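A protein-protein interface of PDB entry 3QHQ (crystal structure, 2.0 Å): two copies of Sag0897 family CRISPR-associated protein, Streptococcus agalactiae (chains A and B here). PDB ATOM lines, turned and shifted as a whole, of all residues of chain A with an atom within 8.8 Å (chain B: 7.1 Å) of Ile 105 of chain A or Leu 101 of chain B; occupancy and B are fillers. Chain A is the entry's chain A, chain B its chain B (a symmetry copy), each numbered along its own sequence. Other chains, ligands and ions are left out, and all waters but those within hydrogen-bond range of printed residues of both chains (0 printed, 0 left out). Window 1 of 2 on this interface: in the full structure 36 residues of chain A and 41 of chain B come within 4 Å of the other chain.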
ATOM      1  N   MET A  97       3.702   6.666 -27.327  1.00  0.00           N
ATOM      2  CA  MET A  97       2.689   7.715 -27.405  1.00  0.00           C
ATOM      3  C   MET A  97       3.040   8.927 -26.544  1.00  0.00           C
ATOM      4  O   MET A  97       2.932  10.063 -27.007  1.00  0.00           O
ATOM      5  CB  MET A  97       1.315   7.168 -27.018  1.00  0.00           C
ATOM      6  CG  MET A  97       0.709   6.241 -28.061  1.00  0.00           C
ATOM      7  SD  MET A  97      -0.695   5.324 -27.419  1.00  0.00           S
ATOM      8  CE  MET A  97      -1.827   6.662 -27.004  1.00  0.00           C
ATOM      9  N   VAL A  98       3.453   8.689 -25.300  1.00  0.00           N
ATOM     10  CA  VAL A  98       3.882   9.776 -24.419  1.00  0.00           C
ATOM     11  C   VAL A  98       5.070  10.523 -25.046  1.00  0.00           C
ATOM     12  O   VAL A  98       5.070  11.750 -25.098  1.00  0.00           O
ATOM     13  CB  VAL A  98       4.245   9.280 -22.990  1.00  0.00           C
ATOM     14  CG1 VAL A  98       4.729  10.431 -22.130  1.00  0.00           C
ATOM     15  CG2 VAL A  98       3.045   8.613 -22.337  1.00  0.00           C
ATOM     16  N   GLU A  99       6.055   9.770 -25.541  1.00  0.00           N
ATOM     17  CA  GLU A  99       7.253  10.345 -26.167  1.00  0.00           C
ATOM     18  C   GLU A  99       6.926  11.200 -27.393  1.00  0.00           C
ATOM     19  O   GLU A  99       7.519  12.266 -27.596  1.00  0.00           O
ATOM     20  CB  GLU A  99       8.262   9.244 -26.527  1.00  0.00           C
ATOM     21  CG  GLU A  99       8.907   8.587 -25.305  1.00  0.00           C
ATOM     22  CD  GLU A  99       9.715   7.342 -25.641  1.00  0.00           C
ATOM     23  OE1 GLU A  99       9.654   6.852 -26.789  1.00  0.00           O
ATOM     24  OE2 GLU A  99      10.414   6.846 -24.740  1.00  0.00           O
ATOM     25  N   LYS A 100       5.986  10.722 -28.207  1.00  0.00           N
ATOM     26  CA  LYS A 100       5.520  11.460 -29.375  1.00  0.00           C
ATOM     27  C   LYS A 100       4.915  12.815 -28.990  1.00  0.00           C
ATOM     28  O   LYS A 100       5.246  13.847 -29.586  1.00  0.00           O
ATOM     29  CB  LYS A 100       4.499  10.630 -30.157  1.00  0.00           C
ATOM     30  CG  LYS A 100       5.084   9.663 -31.183  1.00  0.00           C
ATOM     31  CD  LYS A 100       3.948   8.899 -31.876  1.00  0.00           C
ATOM     32  CE  LYS A 100       4.459   7.863 -32.868  1.00  0.00           C
ATOM     33  NZ  LYS A 100       3.363   6.930 -33.296  1.00  0.00           N
ATOM     34  N   LEU A 101       4.035  12.798 -27.993  1.00  0.00           N
ATOM     35  CA  LEU A 101       3.349  13.996 -27.507  1.00  0.00           C
ATOM     36  C   LEU A 101       4.328  15.003 -26.906  1.00  0.00           C
ATOM     37  O   LEU A 101       4.213  16.209 -27.140  1.00  0.00           O
ATOM     38  CB  LEU A 101       2.275  13.612 -26.481  1.00  0.00           C
ATOM     39  CG  LEU A 101       1.083  12.777 -26.973  1.00  0.00           C
ATOM     40  CD1 LEU A 101       0.422  12.019 -25.818  1.00  0.00           C
ATOM     41  CD2 LEU A 101       0.058  13.628 -27.740  1.00  0.00           C
ATOM     42  N   ALA A 102       5.297  14.492 -26.146  1.00  0.00           N
ATOM     43  CA  ALA A 102       6.345  15.316 -25.561  1.00  0.00           C
ATOM     44  C   ALA A 102       7.200  15.987 -26.633  1.00  0.00           C
ATOM     45  O   ALA A 102       7.600  17.136 -26.471  1.00  0.00           O
ATOM     46  CB  ALA A 102       7.211  14.485 -24.616  1.00  0.00           C
ATOM     47  N   ALA A 103       7.462  15.271 -27.727  1.00  0.00           N
ATOM     48  CA  ALA A 103       8.235  15.805 -28.853  1.00  0.00           C
ATOM     49  C   ALA A 103       7.470  16.878 -29.630  1.00  0.00           C
ATOM     50  O   ALA A 103       8.069  17.841 -30.121  1.00  0.00           O
ATOM     51  CB  ALA A 103       8.674  14.681 -29.790  1.00  0.00           C
ATOM     52  N   THR A 104       6.155  16.714 -29.753  1.00  0.00           N
ATOM     53  CA  THR A 104       5.332  17.739 -30.399  1.00  0.00           C
ATOM     54  C   THR A 104       5.314  19.012 -29.547  1.00  0.00           C
ATOM     55  O   THR A 104       5.523  20.108 -30.069  1.00  0.00           O
ATOM     56  CB  THR A 104       3.904  17.239 -30.713  1.00  0.00           C
ATOM     57  OG1 THR A 104       3.979  15.995 -31.422  1.00  0.00           O
ATOM     58  CG2 THR A 104       3.157  18.248 -31.582  1.00  0.00           C
ATOM     59  N   ILE A 105       5.103  18.860 -28.239  1.00  0.00           N
ATOM     60  CA  ILE A 105       5.215  19.986 -27.302  1.00  0.00           C
ATOM     61  C   ILE A 105       6.595  20.663 -27.414  1.00  0.00           C
ATOM     62  O   ILE A 105       6.680  21.889 -27.516  1.00  0.00           O
ATOM     63  CB  ILE A 105       4.938  19.563 -25.834  1.00  0.00           C
ATOM     64  CG1 ILE A 105       3.468  19.171 -25.654  1.00  0.00           C
ATOM     65  CG2 ILE A 105       5.317  20.687 -24.852  1.00  0.00           C
ATOM     66  CD1 ILE A 105       3.153  18.459 -24.339  1.00  0.00           C
ATOM     67  N   THR A 106       7.656  19.857 -27.413  1.00  0.00           N
ATOM     68  CA  THR A 106       9.030  20.363 -27.548  1.00  0.00           C
ATOM     69  C   THR A 106       9.199  21.230 -28.802  1.00  0.00           C
ATOM     70  O   THR A 106       9.731  22.340 -28.722  1.00  0.00           O
ATOM     71  CB  THR A 106      10.076  19.212 -27.523  1.00  0.00           C
ATOM     72  OG1 THR A 106       9.911  18.455 -26.321  1.00  0.00           O
ATOM     73  CG2 THR A 106      11.502  19.750 -27.570  1.00  0.00           C
ATOM     74  N   GLU A 107       8.727  20.732 -29.945  1.00  0.00           N
ATOM     75  CA  GLU A 107       8.826  21.474 -31.195  1.00  0.00           C
ATOM     76  C   GLU A 107       8.087  22.818 -31.099  1.00  0.00           C
ATOM     77  O   GLU A 107       8.551  23.812 -31.649  1.00  0.00           O
ATOM     78  CB  GLU A 107       8.348  20.632 -32.391  1.00  0.00           C
ATOM     79  CG  GLU A 107       6.978  21.015 -32.951  1.00  0.00           C
ATOM     80  CD  GLU A 107       6.533  20.155 -34.126  1.00  0.00           C
ATOM     81  OE1 GLU A 107       6.458  20.692 -35.253  1.00  0.00           O
ATOM     82  OE2 GLU A 107       6.250  18.952 -33.925  1.00  0.00           O
ATOM     83  N   LEU A 108       6.965  22.849 -30.375  1.00  0.00           N
ATOM     84  CA  LEU A 108       6.218  24.098 -30.180  1.00  0.00           C
ATOM     85  C   LEU A 108       6.972  25.103 -29.286  1.00  0.00           C
ATOM     86  O   LEU A 108       7.090  26.282 -29.640  1.00  0.00           O
ATOM     87  CB  LEU A 108       4.785  23.836 -29.680  1.00  0.00           C
ATOM     88  CG  LEU A 108       3.786  23.203 -30.675  1.00  0.00           C
ATOM     89  CD1 LEU A 108       2.478  22.802 -29.991  1.00  0.00           C
ATOM     90  CD2 LEU A 108       3.488  24.104 -31.883  1.00  0.00           C
ATOM     91  N   ILE A 109       7.488  24.635 -28.150  1.00  0.00           N
ATOM     92  CA  ILE A 109       8.326  25.471 -27.273  1.00  0.00           C
ATOM     93  C   ILE A 109       9.623  25.907 -27.974  1.00  0.00           C
ATOM     94  O   ILE A 109      10.073  27.042 -27.796  1.00  0.00           O
ATOM     95  CB  ILE A 109       8.658  24.772 -25.922  1.00  0.00           C
ATOM     96  CG1 ILE A 109       7.376  24.414 -25.163  1.00  0.00           C
ATOM     97  CG2 ILE A 109       9.561  25.666 -25.042  1.00  0.00           C
ATOM     98  CD1 ILE A 109       7.596  23.417 -24.015  1.00  0.00           C
ATOM     99  N   ALA A 110      10.215  25.012 -28.765  1.00  0.00           N
ATOM    100  CA  ALA A 110      11.422  25.334 -29.537  1.00  0.00           C
ATOM    101  C   ALA A 110      11.191  26.516 -30.473  1.00  0.00           C
ATOM    102  O   ALA A 110      12.059  27.381 -30.618  1.00  0.00           O
ATOM    103  CB  ALA A 110      11.909  24.125 -30.323  1.00  0.00           C
ATOM    104  N   PHE A 111      10.016  26.557 -31.096  1.00  0.00           N
ATOM    105  CA  PHE A 111       9.666  27.667 -31.977  1.00  0.00           C
ATOM    106  C   PHE A 111       9.626  28.990 -31.215  1.00  0.00           C
ATOM    107  O   PHE A 111      10.157  29.992 -31.692  1.00  0.00           O
ATOM    108  CB  PHE A 111       8.342  27.419 -32.711  1.00  0.00           C
ATOM    109  CG  PHE A 111       8.047  28.440 -33.782  1.00  0.00           C
ATOM    110  CD1 PHE A 111       7.129  29.461 -33.555  1.00  0.00           C
ATOM    111  CD2 PHE A 111       8.713  28.398 -35.009  1.00  0.00           C
ATOM    112  CE1 PHE A 111       6.865  30.416 -34.538  1.00  0.00           C
ATOM    113  CE2 PHE A 111       8.460  29.347 -35.994  1.00  0.00           C
ATOM    114  CZ  PHE A 111       7.531  30.358 -35.760  1.00  0.00           C
ATOM    115  N   GLU A 112       9.006  28.984 -30.034  1.00  0.00           N
ATOM    116  CA  GLU A 112       8.954  30.179 -29.188  1.00  0.00           C
ATOM    117  C   GLU A 112      10.341  30.621 -28.720  1.00  0.00           C
ATOM    118  O   GLU A 112      10.594  31.820 -28.587  1.00  0.00           O
ATOM    119  CB  GLU A 112       8.023  29.980 -27.990  1.00  0.00           C
ATOM    120  CG  GLU A 112       6.554  29.754 -28.359  1.00  0.00           C
ATOM    121  CD  GLU A 112       5.978  30.822 -29.289  1.00  0.00           C
ATOM    122  OE1 GLU A 112       6.263  32.027 -29.098  1.00  0.00           O
ATOM    123  OE2 GLU A 112       5.227  30.444 -30.212  1.00  0.00           O
ATOM    124  N   TYR A 122      18.112  24.138 -24.969  1.00  0.00           N
ATOM    125  CA  TYR A 122      17.307  23.324 -24.059  1.00  0.00           C
ATOM    126  C   TYR A 122      17.768  21.869 -24.102  1.00  0.00           C
ATOM    127  O   TYR A 122      18.618  21.507 -24.925  1.00  0.00           O
ATOM    128  CB  TYR A 122      15.812  23.429 -24.411  1.00  0.00           C
ATOM    129  CG  TYR A 122      15.503  23.143 -25.857  1.00  0.00           C
ATOM    130  CD1 TYR A 122      15.383  21.831 -26.323  1.00  0.00           C
ATOM    131  CD2 TYR A 122      15.341  24.183 -26.769  1.00  0.00           C
ATOM    132  CE1 TYR A 122      15.114  21.569 -27.663  1.00  0.00           C
ATOM    133  CE2 TYR A 122      15.069  23.931 -28.107  1.00  0.00           C
ATOM    134  CZ  TYR A 122      14.955  22.626 -28.543  1.00  0.00           C
ATOM    135  OH  TYR A 122      14.689  22.378 -29.866  1.00  0.00           O
ATOM    136  N   ILE A 125      12.161  16.892 -22.655  1.00  0.00           N
ATOM    137  CA  ILE A 125      11.115  16.596 -21.676  1.00  0.00           C
ATOM    138  C   ILE A 125      10.996  15.077 -21.532  1.00  0.00           C
ATOM    139  O   ILE A 125      10.615  14.384 -22.478  1.00  0.00           O
ATOM    140  CB  ILE A 125       9.749  17.218 -22.075  1.00  0.00           C
ATOM    141  CG1 ILE A 125       9.871  18.737 -22.243  1.00  0.00           C
ATOM    142  CG2 ILE A 125       8.671  16.859 -21.033  1.00  0.00           C
ATOM    143  CD1 ILE A 125       8.651  19.415 -22.912  1.00  0.00           C
ATOM    144  N   LEU A 130       7.471  14.535 -16.679  1.00  0.00           N
ATOM    145  CA  LEU A 130       6.034  14.707 -16.857  1.00  0.00           C
ATOM    146  C   LEU A 130       5.243  14.157 -15.669  1.00  0.00           C
ATOM    147  O   LEU A 130       4.315  14.804 -15.177  1.00  0.00           O
ATOM    148  CB  LEU A 130       5.573  14.068 -18.170  1.00  0.00           C
ATOM    149  CG  LEU A 130       6.094  14.762 -19.429  1.00  0.00           C
ATOM    150  CD1 LEU A 130       5.996  13.844 -20.640  1.00  0.00           C
ATOM    151  CD2 LEU A 130       5.328  16.051 -19.660  1.00  0.00           C
ATOM    152  N   PHE B  88       3.247  32.245 -25.457  1.00  0.00           N
ATOM    153  CA  PHE B  88       2.132  31.327 -25.685  1.00  0.00           C
ATOM    154  C   PHE B  88       0.781  31.994 -25.396  1.00  0.00           C
ATOM    155  O   PHE B  88      -0.174  31.825 -26.163  1.00  0.00           O
ATOM    156  CB  PHE B  88       2.291  30.046 -24.859  1.00  0.00           C
ATOM    157  CG  PHE B  88       3.243  29.039 -25.455  1.00  0.00           C
ATOM    158  CD1 PHE B  88       2.980  28.450 -26.689  1.00  0.00           C
ATOM    159  CD2 PHE B  88       4.387  28.659 -24.766  1.00  0.00           C
ATOM    160  CE1 PHE B  88       3.855  27.509 -27.235  1.00  0.00           C
ATOM    161  CE2 PHE B  88       5.268  27.711 -25.295  1.00  0.00           C
ATOM    162  CZ  PHE B  88       5.001  27.133 -26.529  1.00  0.00           C
ATOM    163  N   VAL B  94      -1.858  28.478 -30.489  1.00  0.00           N
ATOM    164  CA  VAL B  94      -0.744  27.594 -30.187  1.00  0.00           C
ATOM    165  C   VAL B  94      -0.788  27.154 -28.726  1.00  0.00           C
ATOM    166  O   VAL B  94      -0.451  26.012 -28.409  1.00  0.00           O
ATOM    167  CB  VAL B  94       0.605  28.262 -30.546  1.00  0.00           C
ATOM    168  CG1 VAL B  94       1.762  27.303 -30.329  1.00  0.00           C
ATOM    169  CG2 VAL B  94       0.572  28.747 -31.998  1.00  0.00           C
ATOM    170  N   LYS B  95      -1.226  28.058 -27.852  1.00  0.00           N
ATOM    171  CA  LYS B  95      -1.414  27.754 -26.432  1.00  0.00           C
ATOM    172  C   LYS B  95      -2.362  26.561 -26.252  1.00  0.00           C
ATOM    173  O   LYS B  95      -2.081  25.650 -25.458  1.00  0.00           O
ATOM    174  CB  LYS B  95      -1.938  28.988 -25.687  1.00  0.00           C
ATOM    175  CG  LYS B  95      -2.150  28.779 -24.194  1.00  0.00           C
ATOM    176  CD  LYS B  95      -2.862  29.963 -23.567  1.00  0.00           C
ATOM    177  CE  LYS B  95      -3.031  29.767 -22.069  1.00  0.00           C
ATOM    178  NZ  LYS B  95      -3.730  30.939 -21.467  1.00  0.00           N
ATOM    179  N   SER B  96      -3.470  26.576 -26.994  1.00  0.00           N
ATOM    180  CA  SER B  96      -4.451  25.492 -26.977  1.00  0.00           C
ATOM    181  C   SER B  96      -3.860  24.166 -27.454  1.00  0.00           C
ATOM    182  O   SER B  96      -4.182  23.114 -26.903  1.00  0.00           O
ATOM    183  CB  SER B  96      -5.676  25.856 -27.822  1.00  0.00           C
ATOM    184  OG  SER B  96      -6.601  24.780 -27.869  1.00  0.00           O
ATOM    185  N   MET B  97      -3.005  24.227 -28.476  1.00  0.00           N
ATOM    186  CA  MET B  97      -2.304  23.038 -28.988  1.00  0.00           C
ATOM    187  C   MET B  97      -1.485  22.383 -27.877  1.00  0.00           C
ATOM    188  O   MET B  97      -1.580  21.181 -27.669  1.00  0.00           O
ATOM    189  CB  MET B  97      -1.361  23.386 -30.145  1.00  0.00           C
ATOM    190  CG  MET B  97      -2.016  23.853 -31.437  1.00  0.00           C
ATOM    191  SD  MET B  97      -0.751  24.384 -32.627  1.00  0.00           S
ATOM    192  CE  MET B  97      -1.794  24.935 -33.979  1.00  0.00           C
ATOM    193  N   VAL B  98      -0.685  23.187 -27.176  1.00  0.00           N
ATOM    194  CA  VAL B  98       0.148  22.694 -26.071  1.00  0.00           C
ATOM    195  C   VAL B  98      -0.719  22.081 -24.970  1.00  0.00           C
ATOM    196  O   VAL B  98      -0.414  21.003 -24.472  1.00  0.00           O
ATOM    197  CB  VAL B  98       1.060  23.792 -25.478  1.00  0.00           C
ATOM    198  CG1 VAL B  98       1.937  23.221 -24.353  1.00  0.00           C
ATOM    199  CG2 VAL B  98       1.948  24.400 -26.568  1.00  0.00           C
ATOM    200  N   GLU B  99      -1.800  22.776 -24.612  1.00  0.00           N
ATOM    201  CA  GLU B  99      -2.733  22.298 -23.593  1.00  0.00           C
ATOM    202  C   GLU B  99      -3.376  20.964 -23.994  1.00  0.00           C
ATOM    203  O   GLU B  99      -3.470  20.051 -23.174  1.00  0.00           O
ATOM    204  CB  GLU B  99      -3.807  23.353 -23.303  1.00  0.00           C
ATOM    205  CG  GLU B  99      -3.322  24.548 -22.468  1.00  0.00           C
ATOM    206  CD  GLU B  99      -4.320  25.704 -22.457  1.00  0.00           C
ATOM    207  OE1 GLU B  99      -5.237  25.722 -23.305  1.00  0.00           O
ATOM    208  OE2 GLU B  99      -4.181  26.608 -21.608  1.00  0.00           O
ATOM    209  N   LYS B 100      -3.805  20.859 -25.252  1.00  0.00           N
ATOM    210  CA  LYS B 100      -4.417  19.625 -25.765  1.00  0.00           C
ATOM    211  C   LYS B 100      -3.437  18.455 -25.683  1.00  0.00           C
ATOM    212  O   LYS B 100      -3.800  17.360 -25.271  1.00  0.00           O
ATOM    213  CB  LYS B 100      -4.898  19.812 -27.206  1.00  0.00           C
ATOM    214  CG  LYS B 100      -6.234  20.519 -27.327  1.00  0.00           C
ATOM    215  CD  LYS B 100      -6.600  20.751 -28.782  1.00  0.00           C
ATOM    216  CE  LYS B 100      -7.807  21.654 -28.894  1.00  0.00           C
ATOM    217  NZ  LYS B 100      -8.152  21.923 -30.317  1.00  0.00           N
ATOM    218  N   LEU B 101      -2.189  18.709 -26.066  1.00  0.00           N
ATOM    219  CA  LEU B 101      -1.129  17.701 -25.970  1.00  0.00           C
ATOM    220  C   LEU B 101      -0.860  17.292 -24.524  1.00  0.00           C
ATOM    221  O   LEU B 101      -0.683  16.100 -24.221  1.00  0.00           O
ATOM    222  CB  LEU B 101       0.162  18.212 -26.638  1.00  0.00           C
ATOM    223  CG  LEU B 101       0.110  18.478 -28.148  1.00  0.00           C
ATOM    224  CD1 LEU B 101       1.279  19.364 -28.606  1.00  0.00           C
ATOM    225  CD2 LEU B 101       0.055  17.182 -28.957  1.00  0.00           C
ATOM    226  N   ALA B 102      -0.840  18.277 -23.628  1.00  0.00           N
ATOM    227  CA  ALA B 102      -0.602  18.010 -22.210  1.00  0.00           C
ATOM    228  C   ALA B 102      -1.744  17.208 -21.579  1.00  0.00           C
ATOM    229  O   ALA B 102      -1.516  16.397 -20.674  1.00  0.00           O
ATOM    230  CB  ALA B 102      -0.372  19.316 -21.448  1.00  0.00           C
ATOM    231  N   ALA B 103      -2.965  17.439 -22.062  1.00  0.00           N
ATOM    232  CA  ALA B 103      -4.146  16.731 -21.558  1.00  0.00           C
ATOM    233  C   ALA B 103      -4.123  15.260 -21.959  1.00  0.00           C
ATOM    234  O   ALA B 103      -4.559  14.402 -21.195  1.00  0.00           O
ATOM    235  CB  ALA B 103      -5.418  17.397 -22.055  1.00  0.00           C
ATOM    236  N   THR B 104      -3.631  14.977 -23.164  1.00  0.00           N
ATOM    237  CA  THR B 104      -3.477  13.602 -23.626  1.00  0.00           C
ATOM    238  C   THR B 104      -2.419  12.884 -22.778  1.00  0.00           C
ATOM    239  O   THR B 104      -2.688  11.814 -22.236  1.00  0.00           O
ATOM    240  CB  THR B 104      -3.161  13.530 -25.144  1.00  0.00           C
ATOM    241  OG1 THR B 104      -4.141  14.281 -25.869  1.00  0.00           O
ATOM    242  CG2 THR B 104      -3.193  12.094 -25.637  1.00  0.00           C
ATOM    243  N   ILE B 105      -1.235  13.488 -22.643  1.00  0.00           N
ATOM    244  CA  ILE B 105      -0.196  12.989 -21.726  1.00  0.00           C
ATOM    245  C   ILE B 105      -0.755  12.703 -20.330  1.00  0.00           C
ATOM    246  O   ILE B 105      -0.522  11.626 -19.754  1.00  0.00           O
ATOM    247  CB  ILE B 105       0.997  13.989 -21.603  1.00  0.00           C
ATOM    248  CG1 ILE B 105       1.808  14.004 -22.895  1.00  0.00           C
ATOM    249  CG2 ILE B 105       1.896  13.625 -20.396  1.00  0.00           C
ATOM    250  CD1 ILE B 105       2.870  15.113 -22.973  1.00  0.00           C
ATOM    251  N   THR B 106      -1.500  13.672 -19.799  1.00  0.00           N
ATOM    252  CA  THR B 106      -2.094  13.569 -18.464  1.00  0.00           C
ATOM    253  C   THR B 106      -2.952  12.310 -18.294  1.00  0.00           C
ATOM    254  O   THR B 106      -2.824  11.606 -17.291  1.00  0.00           O
ATOM    255  CB  THR B 106      -2.931  14.824 -18.148  1.00  0.00           C
ATOM    256  OG1 THR B 106      -2.055  15.954 -18.059  1.00  0.00           O
ATOM    257  CG2 THR B 106      -3.701  14.668 -16.832  1.00  0.00           C
ATOM    258  N   ILE B 125      -0.420  19.322 -15.575  1.00  0.00           N
ATOM    259  CA  ILE B 125       0.821  19.708 -16.245  1.00  0.00           C
ATOM    260  C   ILE B 125       0.583  21.030 -16.976  1.00  0.00           C
ATOM    261  O   ILE B 125      -0.210  21.095 -17.921  1.00  0.00           O
ATOM    262  CB  ILE B 125       1.312  18.630 -17.232  1.00  0.00           C
ATOM    263  CG1 ILE B 125       1.606  17.318 -16.492  1.00  0.00           C
ATOM    264  CG2 ILE B 125       2.559  19.116 -17.976  1.00  0.00           C
ATOM    265  CD1 ILE B 125       1.793  16.114 -17.393  1.00  0.00           C
ATOM    266  N   ILE B 127       1.849  24.736 -18.945  1.00  0.00           N
ATOM    267  CA  ILE B 127       2.803  25.180 -19.955  1.00  0.00           C
ATOM    268  C   ILE B 127       4.127  25.594 -19.311  1.00  0.00           C
ATOM    269  O   ILE B 127       5.197  25.235 -19.807  1.00  0.00           O
ATOM    270  CB  ILE B 127       2.226  26.318 -20.848  1.00  0.00           C
ATOM    271  CG1 ILE B 127       1.048  25.782 -21.669  1.00  0.00           C
ATOM    272  CG2 ILE B 127       3.314  26.892 -21.760  1.00  0.00           C
ATOM    273  CD1 ILE B 127       0.301  26.828 -22.489  1.00  0.00           C
ATOM    274  N   LEU B 130       6.131  22.657 -18.432  1.00  0.00           N
ATOM    275  CA  LEU B 130       6.703  22.048 -19.635  1.00  0.00           C
ATOM    276  C   LEU B 130       7.973  22.772 -20.074  1.00  0.00           C
ATOM    277  O   LEU B 130       8.971  22.134 -20.429  1.00  0.00           O
ATOM    278  CB  LEU B 130       5.670  21.999 -20.769  1.00  0.00           C
ATOM    279  CG  LEU B 130       4.501  21.028 -20.529  1.00  0.00           C
ATOM    280  CD1 LEU B 130       3.331  21.326 -21.458  1.00  0.00           C
ATOM    281  CD2 LEU B 130       4.954  19.579 -20.677  1.00  0.00           C
ATOM    282  N   ILE B 131       7.933  24.103 -20.028  1.00  0.00           N
ATOM    283  CA  ILE B 131       9.096  24.937 -20.353  1.00  0.00           C
ATOM    284  C   ILE B 131      10.264  24.657 -19.398  1.00  0.00           C
ATOM    285  O   ILE B 131      11.405  24.484 -19.842  1.00  0.00           O
ATOM    286  CB  ILE B 131       8.724  26.440 -20.343  1.00  0.00           C
ATOM    287  CG1 ILE B 131       7.729  26.745 -21.469  1.00  0.00           C
ATOM    288  CG2 ILE B 131       9.982  27.319 -20.474  1.00  0.00           C
ATOM    289  CD1 ILE B 131       6.981  28.060 -21.304  1.00  0.00           C
ATOM    290  N   LEU B 134      11.750  21.266 -19.982  1.00  0.00           N
ATOM    291  CA  LEU B 134      12.553  21.294 -21.206  1.00  0.00           C
ATOM    292  C   LEU B 134      13.971  21.826 -20.959  1.00  0.00           C
ATOM    293  O   LEU B 134      14.870  21.598 -21.767  1.00  0.00           O
ATOM    294  CB  LEU B 134      11.844  22.095 -22.306  1.00  0.00           C
ATOM    295  CG  LEU B 134      12.369  21.974 -23.748  1.00  0.00           C
ATOM    296  CD1 LEU B 134      12.719  20.538 -24.145  1.00  0.00           C
ATOM    297  CD2 LEU B 134      11.353  22.556 -24.718  1.00  0.00           C
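Leu 101 of chain B touches its own counterpart, Leu 101 of chain A.
Ile 105 of chain B touches its own counterpart, Ile 105 of chain A.
Ile 105 of chain A touches Leu 130 of chain B, but with the chains exchanged Leu 130 of chain A does not touch Ile 105 of chain B (4.1 Å).
Leu 130 of chain B touches its own counterpart, Leu 130 of chain A.
Positions printed for both chains: 97, 98, 99, 100, 101, 102, 103, 104, 105, 106, 125 and 130.
Of the 21 pairs that touch across the chains among the printed residues, 9 have their exchanged pair printed and touching as well.
Printed residues of chain B that touch a printed residue of chain A: Phe 88, Val 94, Met 97, Val 98, Leu 101, Thr 104, Ile 105, Ile 125, Leu 130 and Leu 134.
Of the 19 printed residues of chain A, 10 touch a printed residue of chain B.
Hydrophobic or aromatic side chains of chain A within 4 Å of the printed part of chain B: Leu 101, Ile 105, Leu 108, Ile 109, Tyr 122, Ile 125 and Leu 130.
O of Lys 100 of chain A sits at hydrogen-bond distance from OG1 of Thr 104 of chain A, 3.1 Å away.
OG1 of Thr 106 of chain A lies within hydrogen-bond range of O of Ala 102 of chain A (2.7 Å).
The backbone carbonyl oxygen (O) of Lys 100 of chain B is in hydrogen-bond range of the side-chain hydroxyl (OG1) of Thr 104 of chain B, 3.2 Å away.
Among the printed residues, merely in contact across the chains: Leu 101 of chain A with Leu 101 of chain B (3.8 Å), Leu 101 of chain A with Thr 104 of chain B (3.6 Å), Leu 101 of chain A with Ile 105 of chain B (3.6 Å), Thr 104 of chain A with Leu 101 of chain B (3.7 Å), Ile 105 of chain A with Leu 101 of chain B (3.6 Å), Ile 105 of chain A with Ile 105 of chain B (3.6 Å), Ile 105 of chain A with Leu 130 of chain B (3.98 Å), Thr 106 of chain A with Leu 134 of chain B (3.7 Å), Leu 108 of chain A with Phe 88 of chain B (3.8 Å), Leu 108 of chain A with Val 94 of chain B (3.95 Å), Leu 108 of chain A with Met 97 of chain B (3.9 Å), Leu 108 of chain A with Val 98 of chain B (3.8 Å), Leu 108 of chain A with Leu 101 of chain B (3.9 Å), Ile 109 of chain A with Phe 88 of chain B (3.8 Å), Ile 109 of chain A with Leu 134 of chain B (3.6 Å), Glu 112 of chain A with Phe 88 of chain B (3.6 Å), Tyr 122 of chain A with Leu 134 of chain B (3.4 Å), Ile 125 of chain A with Leu 130 of chain B (3.7 Å), Ile 125 of chain A with Leu 134 of chain B (3.8 Å), Leu 130 of chain A with Ile 125 of chain B (3.6 Å) and Leu 130 of chain A with Leu 130 of chain B (3.7 Å).
Of the printed residues of chain B, Thr 104 of chain A touches Leu 101.
Of the printed residues of chain B, Ile 105 of chain A touches Leu 101, Ile 105 and Leu 130.
Of the printed residues of chain B, Thr 106 of chain A touches Leu 134.
Leu 101 of chain B touches four residues of chain A.
No residue of chain A comes within 4 Å of Ala 102 of chain B.
The nearest printed residue of chain B that does not touch Ile 105 of chain A is Ala 102 of chain B (4.1 Å).
The nearest residue of chain A that does not touch Leu 101 of chain B is Lys 100 of chain A (6.2 Å).
The nearest printed residue of chain A that does not touch Val 94 of chain B is Glu 112 of chain A (4.7 Å).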
